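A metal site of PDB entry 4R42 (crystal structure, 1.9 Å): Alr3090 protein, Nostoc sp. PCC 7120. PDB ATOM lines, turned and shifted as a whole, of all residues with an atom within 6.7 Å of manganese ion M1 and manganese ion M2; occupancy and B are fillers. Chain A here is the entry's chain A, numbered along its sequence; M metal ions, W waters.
OE1 of Glu 64 sits at hydrogen-bond distance from NE2 of His 166 (2.8 Å).
The backbone NH (N) of Glu 35 sits at hydrogen-bond distance from the backbone carbonyl oxygen (O) of Gln 28 (2.9 Å).
A ring nitrogen (ND1) of His 166 lies close to the backbone carbonyl oxygen of Arg 162, 3.4 Å away.
The backbone carbonyl oxygen (O) of Glu 163 lies within hydrogen-bond range of the side-chain hydroxyl (OG1) of Thr 167 (2.8 Å).
NE2 of His 68 lies within hydrogen-bond range of OE2 of Glu 64, 2.9 Å away.
The side-chain carboxylate (OE2) of Glu 133 lies close to the side-chain hydroxyl (OH) of Tyr 42, 2.6 Å away.
OE1 of Glu 35 sits close to OH of Tyr 140, at 2.6 Å.
The nearest printed residue that does not touch manganese ion M1 is Tyr 42 (4.4 Å).
Of the 22 residues printed, 4 come within 4 Å of manganese ion M2.
Manganese ion M1 is bound by the side-chain carboxylate (OE2) of Glu 65 (2.1 Å), the side-chain carboxylate (OE1) of Glu 163 (2.1 Å), water W2 (2.2 Å), the side-chain carboxylate (OE2) of Glu 133 (2.3 Å), a ring nitrogen (ND1) of His 166 (2.3 Å) and the side-chain carboxylate (OE1) of Glu 133 (2.3 Å).
Manganese ion M1 has six donor atoms within binding distance.
Manganese ion M2 is bound by OE2 of Glu 163 (2.1 Å), OE1 of Glu 65 (2.1 Å), OE2 of Glu 35 (2.2 Å), ND1 of His 68 (2.3 Å), OE1 of Glu 35 (2.4 Å) and water W1 (2.5 Å).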
ATOM      1  N   GLN A  28     -17.429 -30.651 -22.511  1.00  0.00           N
ATOM      2  CA  GLN A  28     -17.572 -29.774 -23.673  1.00  0.00           C
ATOM      3  C   GLN A  28     -17.277 -30.511 -24.982  1.00  0.00           C
ATOM      4  O   GLN A  28     -17.382 -29.923 -26.064  1.00  0.00           O
ATOM      5  CB  GLN A  28     -16.696 -28.524 -23.526  1.00  0.00           C
ATOM      6  CG  GLN A  28     -17.205 -27.546 -22.454  1.00  0.00           C
ATOM      7  CD  GLN A  28     -18.701 -27.278 -22.552  1.00  0.00           C
ATOM      8  OE1 GLN A  28     -19.513 -27.955 -21.909  1.00  0.00           O
ATOM      9  NE2 GLN A  28     -19.073 -26.312 -23.373  1.00  0.00           N
ATOM     10  N   GLY A  34     -22.040 -29.238 -24.355  1.00  0.00           N
ATOM     11  CA  GLY A  34     -20.842 -29.253 -25.175  1.00  0.00           C
ATOM     12  C   GLY A  34     -20.966 -28.874 -26.632  1.00  0.00           C
ATOM     13  O   GLY A  34     -22.036 -28.494 -27.122  1.00  0.00           O
ATOM     14  N   GLU A  35     -19.841 -29.004 -27.331  1.00  0.00           N
ATOM     15  CA  GLU A  35     -19.699 -28.504 -28.670  1.00  0.00           C
ATOM     16  C   GLU A  35     -20.437 -29.364 -29.691  1.00  0.00           C
ATOM     17  O   GLU A  35     -20.895 -28.838 -30.701  1.00  0.00           O
ATOM     18  CB  GLU A  35     -18.224 -28.410 -29.051  1.00  0.00           C
ATOM     19  CG  GLU A  35     -17.434 -27.440 -28.187  1.00  0.00           C
ATOM     20  CD  GLU A  35     -17.879 -26.000 -28.346  1.00  0.00           C
ATOM     21  OE1 GLU A  35     -17.465 -25.139 -27.537  1.00  0.00           O
ATOM     22  OE2 GLU A  35     -18.633 -25.707 -29.307  1.00  0.00           O
ATOM     23  N   ALA A  38     -24.040 -28.185 -29.523  1.00  0.00           N
ATOM     24  CA  ALA A  38     -24.246 -26.916 -30.185  1.00  0.00           C
ATOM     25  C   ALA A  38     -24.244 -27.111 -31.705  1.00  0.00           C
ATOM     26  O   ALA A  38     -25.181 -26.679 -32.387  1.00  0.00           O
ATOM     27  CB  ALA A  38     -23.178 -25.893 -29.764  1.00  0.00           C
ATOM     28  N   TYR A  42     -27.795 -26.604 -33.996  1.00  0.00           N
ATOM     29  CA  TYR A  42     -27.949 -25.513 -34.950  1.00  0.00           C
ATOM     30  C   TYR A  42     -28.013 -26.074 -36.363  1.00  0.00           C
ATOM     31  O   TYR A  42     -28.775 -25.587 -37.191  1.00  0.00           O
ATOM     32  CB  TYR A  42     -26.811 -24.495 -34.817  1.00  0.00           C
ATOM     33  CG  TYR A  42     -26.556 -24.032 -33.399  1.00  0.00           C
ATOM     34  CD1 TYR A  42     -27.570 -24.083 -32.438  1.00  0.00           C
ATOM     35  CD2 TYR A  42     -25.317 -23.554 -33.008  1.00  0.00           C
ATOM     36  CE1 TYR A  42     -27.322 -23.693 -31.133  1.00  0.00           C
ATOM     37  CE2 TYR A  42     -25.063 -23.171 -31.708  1.00  0.00           C
ATOM     38  CZ  TYR A  42     -26.075 -23.245 -30.774  1.00  0.00           C
ATOM     39  OH  TYR A  42     -25.851 -22.858 -29.472  1.00  0.00           O
ATOM     40  N   ILE A  61     -22.666 -20.608 -37.595  1.00  0.00           N
ATOM     41  CA  ILE A  61     -22.336 -20.879 -36.196  1.00  0.00           C
ATOM     42  C   ILE A  61     -22.092 -22.389 -35.964  1.00  0.00           C
ATOM     43  O   ILE A  61     -21.131 -22.748 -35.295  1.00  0.00           O
ATOM     44  CB  ILE A  61     -23.448 -20.372 -35.243  1.00  0.00           C
ATOM     45  CG1 ILE A  61     -23.590 -18.850 -35.394  1.00  0.00           C
ATOM     46  CG2 ILE A  61     -23.120 -20.748 -33.803  1.00  0.00           C
ATOM     47  CD1 ILE A  61     -24.773 -18.235 -34.613  1.00  0.00           C
ATOM     48  N   GLU A  64     -18.623 -23.231 -36.872  1.00  0.00           N
ATOM     49  CA  GLU A  64     -17.681 -22.788 -35.838  1.00  0.00           C
ATOM     50  C   GLU A  64     -17.694 -23.731 -34.638  1.00  0.00           C
ATOM     51  O   GLU A  64     -16.650 -23.993 -34.052  1.00  0.00           O
ATOM     52  CB  GLU A  64     -17.971 -21.367 -35.348  1.00  0.00           C
ATOM     53  CG  GLU A  64     -16.827 -20.880 -34.474  1.00  0.00           C
ATOM     54  CD  GLU A  64     -16.993 -19.501 -33.886  1.00  0.00           C
ATOM     55  OE1 GLU A  64     -17.940 -18.783 -34.253  1.00  0.00           O
ATOM     56  OE2 GLU A  64     -16.145 -19.126 -33.051  1.00  0.00           O
ATOM     57  N   GLU A  65     -18.878 -24.216 -34.242  1.00  0.00           N
ATOM     58  CA  GLU A  65     -18.951 -25.122 -33.104  1.00  0.00           C
ATOM     59  C   GLU A  65     -18.187 -26.425 -33.376  1.00  0.00           C
ATOM     60  O   GLU A  65     -17.556 -26.980 -32.478  1.00  0.00           O
ATOM     61  CB  GLU A  65     -20.416 -25.438 -32.733  1.00  0.00           C
ATOM     62  CG  GLU A  65     -21.290 -24.213 -32.458  1.00  0.00           C
ATOM     63  CD  GLU A  65     -20.967 -23.443 -31.166  1.00  0.00           C
ATOM     64  OE1 GLU A  65     -19.811 -23.456 -30.698  1.00  0.00           O
ATOM     65  OE2 GLU A  65     -21.884 -22.791 -30.630  1.00  0.00           O
ATOM     66  N   PHE A  66     -18.221 -26.890 -34.617  1.00  0.00           N
ATOM     67  CA  PHE A  66     -17.426 -28.061 -34.998  1.00  0.00           C
ATOM     68  C   PHE A  66     -15.945 -27.756 -34.854  1.00  0.00           C
ATOM     69  O   PHE A  66     -15.153 -28.622 -34.478  1.00  0.00           O
ATOM     70  CB  PHE A  66     -17.720 -28.495 -36.439  1.00  0.00           C
ATOM     71  CG  PHE A  66     -18.952 -29.363 -36.603  1.00  0.00           C
ATOM     72  CD1 PHE A  66     -19.128 -30.508 -35.830  1.00  0.00           C
ATOM     73  CD2 PHE A  66     -19.919 -29.031 -37.533  1.00  0.00           C
ATOM     74  CE1 PHE A  66     -20.263 -31.315 -36.010  1.00  0.00           C
ATOM     75  CE2 PHE A  66     -21.053 -29.829 -37.702  1.00  0.00           C
ATOM     76  CZ  PHE A  66     -21.215 -30.967 -36.945  1.00  0.00           C
ATOM     77  N   HIS A  68     -14.773 -25.633 -32.649  1.00  0.00           N
ATOM     78  CA  HIS A  68     -14.584 -25.655 -31.205  1.00  0.00           C
ATOM     79  C   HIS A  68     -14.450 -27.095 -30.699  1.00  0.00           C
ATOM     80  O   HIS A  68     -13.632 -27.393 -29.823  1.00  0.00           O
ATOM     81  CB  HIS A  68     -15.755 -25.006 -30.460  1.00  0.00           C
ATOM     82  CG  HIS A  68     -15.919 -23.529 -30.698  1.00  0.00           C
ATOM     83  ND1 HIS A  68     -16.919 -22.797 -30.100  1.00  0.00           N
ATOM     84  CD2 HIS A  68     -15.209 -22.651 -31.452  1.00  0.00           C
ATOM     85  CE1 HIS A  68     -16.834 -21.536 -30.495  1.00  0.00           C
ATOM     86  NE2 HIS A  68     -15.804 -21.415 -31.307  1.00  0.00           N
ATOM     87  N   LEU A  69     -15.273 -27.995 -31.238  1.00  0.00           N
ATOM     88  CA  LEU A  69     -15.242 -29.407 -30.851  1.00  0.00           C
ATOM     89  C   LEU A  69     -13.852 -29.979 -31.115  1.00  0.00           C
ATOM     90  O   LEU A  69     -13.316 -30.739 -30.310  1.00  0.00           O
ATOM     91  CB  LEU A  69     -16.303 -30.197 -31.616  1.00  0.00           C
ATOM     92  CG  LEU A  69     -16.419 -31.689 -31.305  1.00  0.00           C
ATOM     93  CD1 LEU A  69     -16.881 -31.944 -29.872  1.00  0.00           C
ATOM     94  CD2 LEU A  69     -17.366 -32.316 -32.294  1.00  0.00           C
ATOM     95  N   ALA A 132     -28.814 -22.954 -24.945  1.00  0.00           N
ATOM     96  CA  ALA A 132     -27.699 -23.858 -25.165  1.00  0.00           C
ATOM     97  C   ALA A 132     -26.409 -23.098 -24.906  1.00  0.00           C
ATOM     98  O   ALA A 132     -25.532 -23.585 -24.176  1.00  0.00           O
ATOM     99  CB  ALA A 132     -27.725 -24.422 -26.591  1.00  0.00           C
ATOM    100  N   GLU A 133     -26.302 -21.905 -25.492  1.00  0.00           N
ATOM    101  CA  GLU A 133     -25.140 -21.052 -25.306  1.00  0.00           C
ATOM    102  C   GLU A 133     -24.925 -20.739 -23.826  1.00  0.00           C
ATOM    103  O   GLU A 133     -23.792 -20.592 -23.382  1.00  0.00           O
ATOM    104  CB  GLU A 133     -25.266 -19.746 -26.095  1.00  0.00           C
ATOM    105  CG  GLU A 133     -25.297 -19.910 -27.615  1.00  0.00           C
ATOM    106  CD  GLU A 133     -23.978 -20.385 -28.184  1.00  0.00           C
ATOM    107  OE1 GLU A 133     -22.929 -20.060 -27.608  1.00  0.00           O
ATOM    108  OE2 GLU A 133     -24.002 -21.078 -29.236  1.00  0.00           O
ATOM    109  N   ALA A 136     -23.371 -23.751 -22.254  1.00  0.00           N
ATOM    110  CA  ALA A 136     -21.991 -23.861 -22.726  1.00  0.00           C
ATOM    111  C   ALA A 136     -21.077 -22.865 -22.007  1.00  0.00           C
ATOM    112  O   ALA A 136     -19.995 -23.223 -21.534  1.00  0.00           O
ATOM    113  CB  ALA A 136     -21.918 -23.662 -24.243  1.00  0.00           C
ATOM    114  N   TYR A 140     -17.964 -23.718 -19.381  1.00  0.00           N
ATOM    115  CA  TYR A 140     -16.616 -23.193 -19.620  1.00  0.00           C
ATOM    116  C   TYR A 140     -16.149 -22.417 -18.399  1.00  0.00           C
ATOM    117  O   TYR A 140     -14.987 -22.557 -18.016  1.00  0.00           O
ATOM    118  CB  TYR A 140     -16.558 -22.313 -20.887  1.00  0.00           C
ATOM    119  CG  TYR A 140     -16.360 -23.124 -22.162  1.00  0.00           C
ATOM    120  CD1 TYR A 140     -15.311 -24.034 -22.260  1.00  0.00           C
ATOM    121  CD2 TYR A 140     -17.231 -23.005 -23.243  1.00  0.00           C
ATOM    122  CE1 TYR A 140     -15.128 -24.802 -23.406  1.00  0.00           C
ATOM    123  CE2 TYR A 140     -17.059 -23.768 -24.407  1.00  0.00           C
ATOM    124  CZ  TYR A 140     -16.011 -24.669 -24.477  1.00  0.00           C
ATOM    125  OH  TYR A 140     -15.814 -25.447 -25.591  1.00  0.00           O
ATOM    126  N   LEU A 159     -12.992 -19.832 -26.004  1.00  0.00           N
ATOM    127  CA  LEU A 159     -14.197 -20.572 -26.318  1.00  0.00           C
ATOM    128  C   LEU A 159     -15.394 -19.956 -25.597  1.00  0.00           C
ATOM    129  O   LEU A 159     -16.459 -19.796 -26.167  1.00  0.00           O
ATOM    130  CB  LEU A 159     -14.027 -22.046 -25.951  1.00  0.00           C
ATOM    131  CG  LEU A 159     -12.968 -22.773 -26.780  1.00  0.00           C
ATOM    132  CD1 LEU A 159     -12.597 -24.102 -26.154  1.00  0.00           C
ATOM    133  CD2 LEU A 159     -13.457 -22.953 -28.225  1.00  0.00           C
ATOM    134  N   ARG A 162     -16.437 -16.809 -27.391  1.00  0.00           N
ATOM    135  CA  ARG A 162     -17.209 -17.109 -28.599  1.00  0.00           C
ATOM    136  C   ARG A 162     -18.674 -17.500 -28.288  1.00  0.00           C
ATOM    137  O   ARG A 162     -19.554 -17.242 -29.116  1.00  0.00           O
ATOM    138  CB  ARG A 162     -16.524 -18.210 -29.416  1.00  0.00           C
ATOM    139  CG  ARG A 162     -15.126 -17.816 -29.956  1.00  0.00           C
ATOM    140  CD  ARG A 162     -15.165 -16.516 -30.781  1.00  0.00           C
ATOM    141  NE  ARG A 162     -16.160 -16.632 -31.840  1.00  0.00           N
ATOM    142  CZ  ARG A 162     -16.763 -15.617 -32.458  1.00  0.00           C
ATOM    143  NH1 ARG A 162     -16.495 -14.359 -32.133  1.00  0.00           N
ATOM    144  NH2 ARG A 162     -17.647 -15.877 -33.414  1.00  0.00           N
ATOM    145  N   GLU A 163     -18.961 -18.095 -27.129  1.00  0.00           N
ATOM    146  CA  GLU A 163     -20.345 -18.405 -26.819  1.00  0.00           C
ATOM    147  C   GLU A 163     -21.116 -17.116 -26.430  1.00  0.00           C
ATOM    148  O   GLU A 163     -22.326 -17.021 -26.659  1.00  0.00           O
ATOM    149  CB  GLU A 163     -20.484 -19.456 -25.697  1.00  0.00           C
ATOM    150  CG  GLU A 163     -19.585 -20.733 -25.763  1.00  0.00           C
ATOM    151  CD  GLU A 163     -19.427 -21.435 -27.136  1.00  0.00           C
ATOM    152  OE1 GLU A 163     -19.924 -20.981 -28.193  1.00  0.00           O
ATOM    153  OE2 GLU A 163     -18.743 -22.498 -27.129  1.00  0.00           O
ATOM    154  N   ILE A 164     -20.438 -16.124 -25.855  1.00  0.00           N
ATOM    155  CA  ILE A 164     -21.075 -14.831 -25.631  1.00  0.00           C
ATOM    156  C   ILE A 164     -21.393 -14.220 -26.996  1.00  0.00           C
ATOM    157  O   ILE A 164     -22.478 -13.686 -27.201  1.00  0.00           O
ATOM    158  CB  ILE A 164     -20.177 -13.906 -24.788  1.00  0.00           C
ATOM    159  CG1 ILE A 164     -20.065 -14.475 -23.368  1.00  0.00           C
ATOM    160  CG2 ILE A 164     -20.719 -12.477 -24.730  1.00  0.00           C
ATOM    161  CD1 ILE A 164     -18.913 -13.935 -22.559  1.00  0.00           C
ATOM    162  N   HIS A 166     -21.916 -15.788 -29.878  1.00  0.00           N
ATOM    163  CA  HIS A 166     -23.032 -16.513 -30.445  1.00  0.00           C
ATOM    164  C   HIS A 166     -24.334 -16.115 -29.788  1.00  0.00           C
ATOM    165  O   HIS A 166     -25.364 -16.015 -30.461  1.00  0.00           O
ATOM    166  CB  HIS A 166     -22.838 -18.021 -30.294  1.00  0.00           C
ATOM    167  CG  HIS A 166     -21.672 -18.549 -31.030  1.00  0.00           C
ATOM    168  ND1 HIS A 166     -21.145 -19.801 -30.791  1.00  0.00           N
ATOM    169  CD2 HIS A 166     -20.930 -18.013 -32.034  1.00  0.00           C
ATOM    170  CE1 HIS A 166     -20.121 -20.009 -31.603  1.00  0.00           C
ATOM    171  NE2 HIS A 166     -19.963 -18.936 -32.356  1.00  0.00           N
ATOM    172  N   THR A 167     -24.307 -15.938 -28.479  1.00  0.00           N
ATOM    173  CA  THR A 167     -25.516 -15.504 -27.766  1.00  0.00           C
ATOM    174  C   THR A 167     -26.030 -14.198 -28.379  1.00  0.00           C
ATOM    175  O   THR A 167     -27.221 -14.023 -28.616  1.00  0.00           O
ATOM    176  CB  THR A 167     -25.256 -15.276 -26.258  1.00  0.00           C
ATOM    177  OG1 THR A 167     -24.843 -16.517 -25.667  1.00  0.00           O
ATOM    178  CG2 THR A 167     -26.528 -14.771 -25.551  1.00  0.00           C
ATOM    179  N   PHE A 170     -27.664 -14.888 -31.797  1.00  0.00           N
ATOM    180  CA  PHE A 170     -29.028 -15.397 -31.619  1.00  0.00           C
ATOM    181  C   PHE A 170     -29.998 -14.339 -31.095  1.00  0.00           C
ATOM    182  O   PHE A 170     -31.179 -14.301 -31.480  1.00  0.00           O
ATOM    183  CB  PHE A 170     -29.005 -16.619 -30.672  1.00  0.00           C
ATOM    184  CG  PHE A 170     -28.323 -17.820 -31.268  1.00  0.00           C
ATOM    185  CD1 PHE A 170     -28.697 -18.321 -32.500  1.00  0.00           C
ATOM    186  CD2 PHE A 170     -27.289 -18.448 -30.593  1.00  0.00           C
ATOM    187  CE1 PHE A 170     -28.067 -19.424 -33.044  1.00  0.00           C
ATOM    188  CE2 PHE A 170     -26.650 -19.550 -31.147  1.00  0.00           C
ATOM    189  CZ  PHE A 170     -27.041 -20.031 -32.365  1.00  0.00           C
HETATM  190 MN    MN M   1     -21.748 -21.318 -29.173  1.00  0.00          MN
HETATM  191 MN    MN M   2     -18.677 -23.567 -28.882  1.00  0.00          MN
HETATM  192  O   HOH W   1     -20.647 -24.634 -27.741  1.00  0.00           O
HETATM  193  O   HOH W   2     -22.061 -22.890 -27.640  1.00  0.00           O
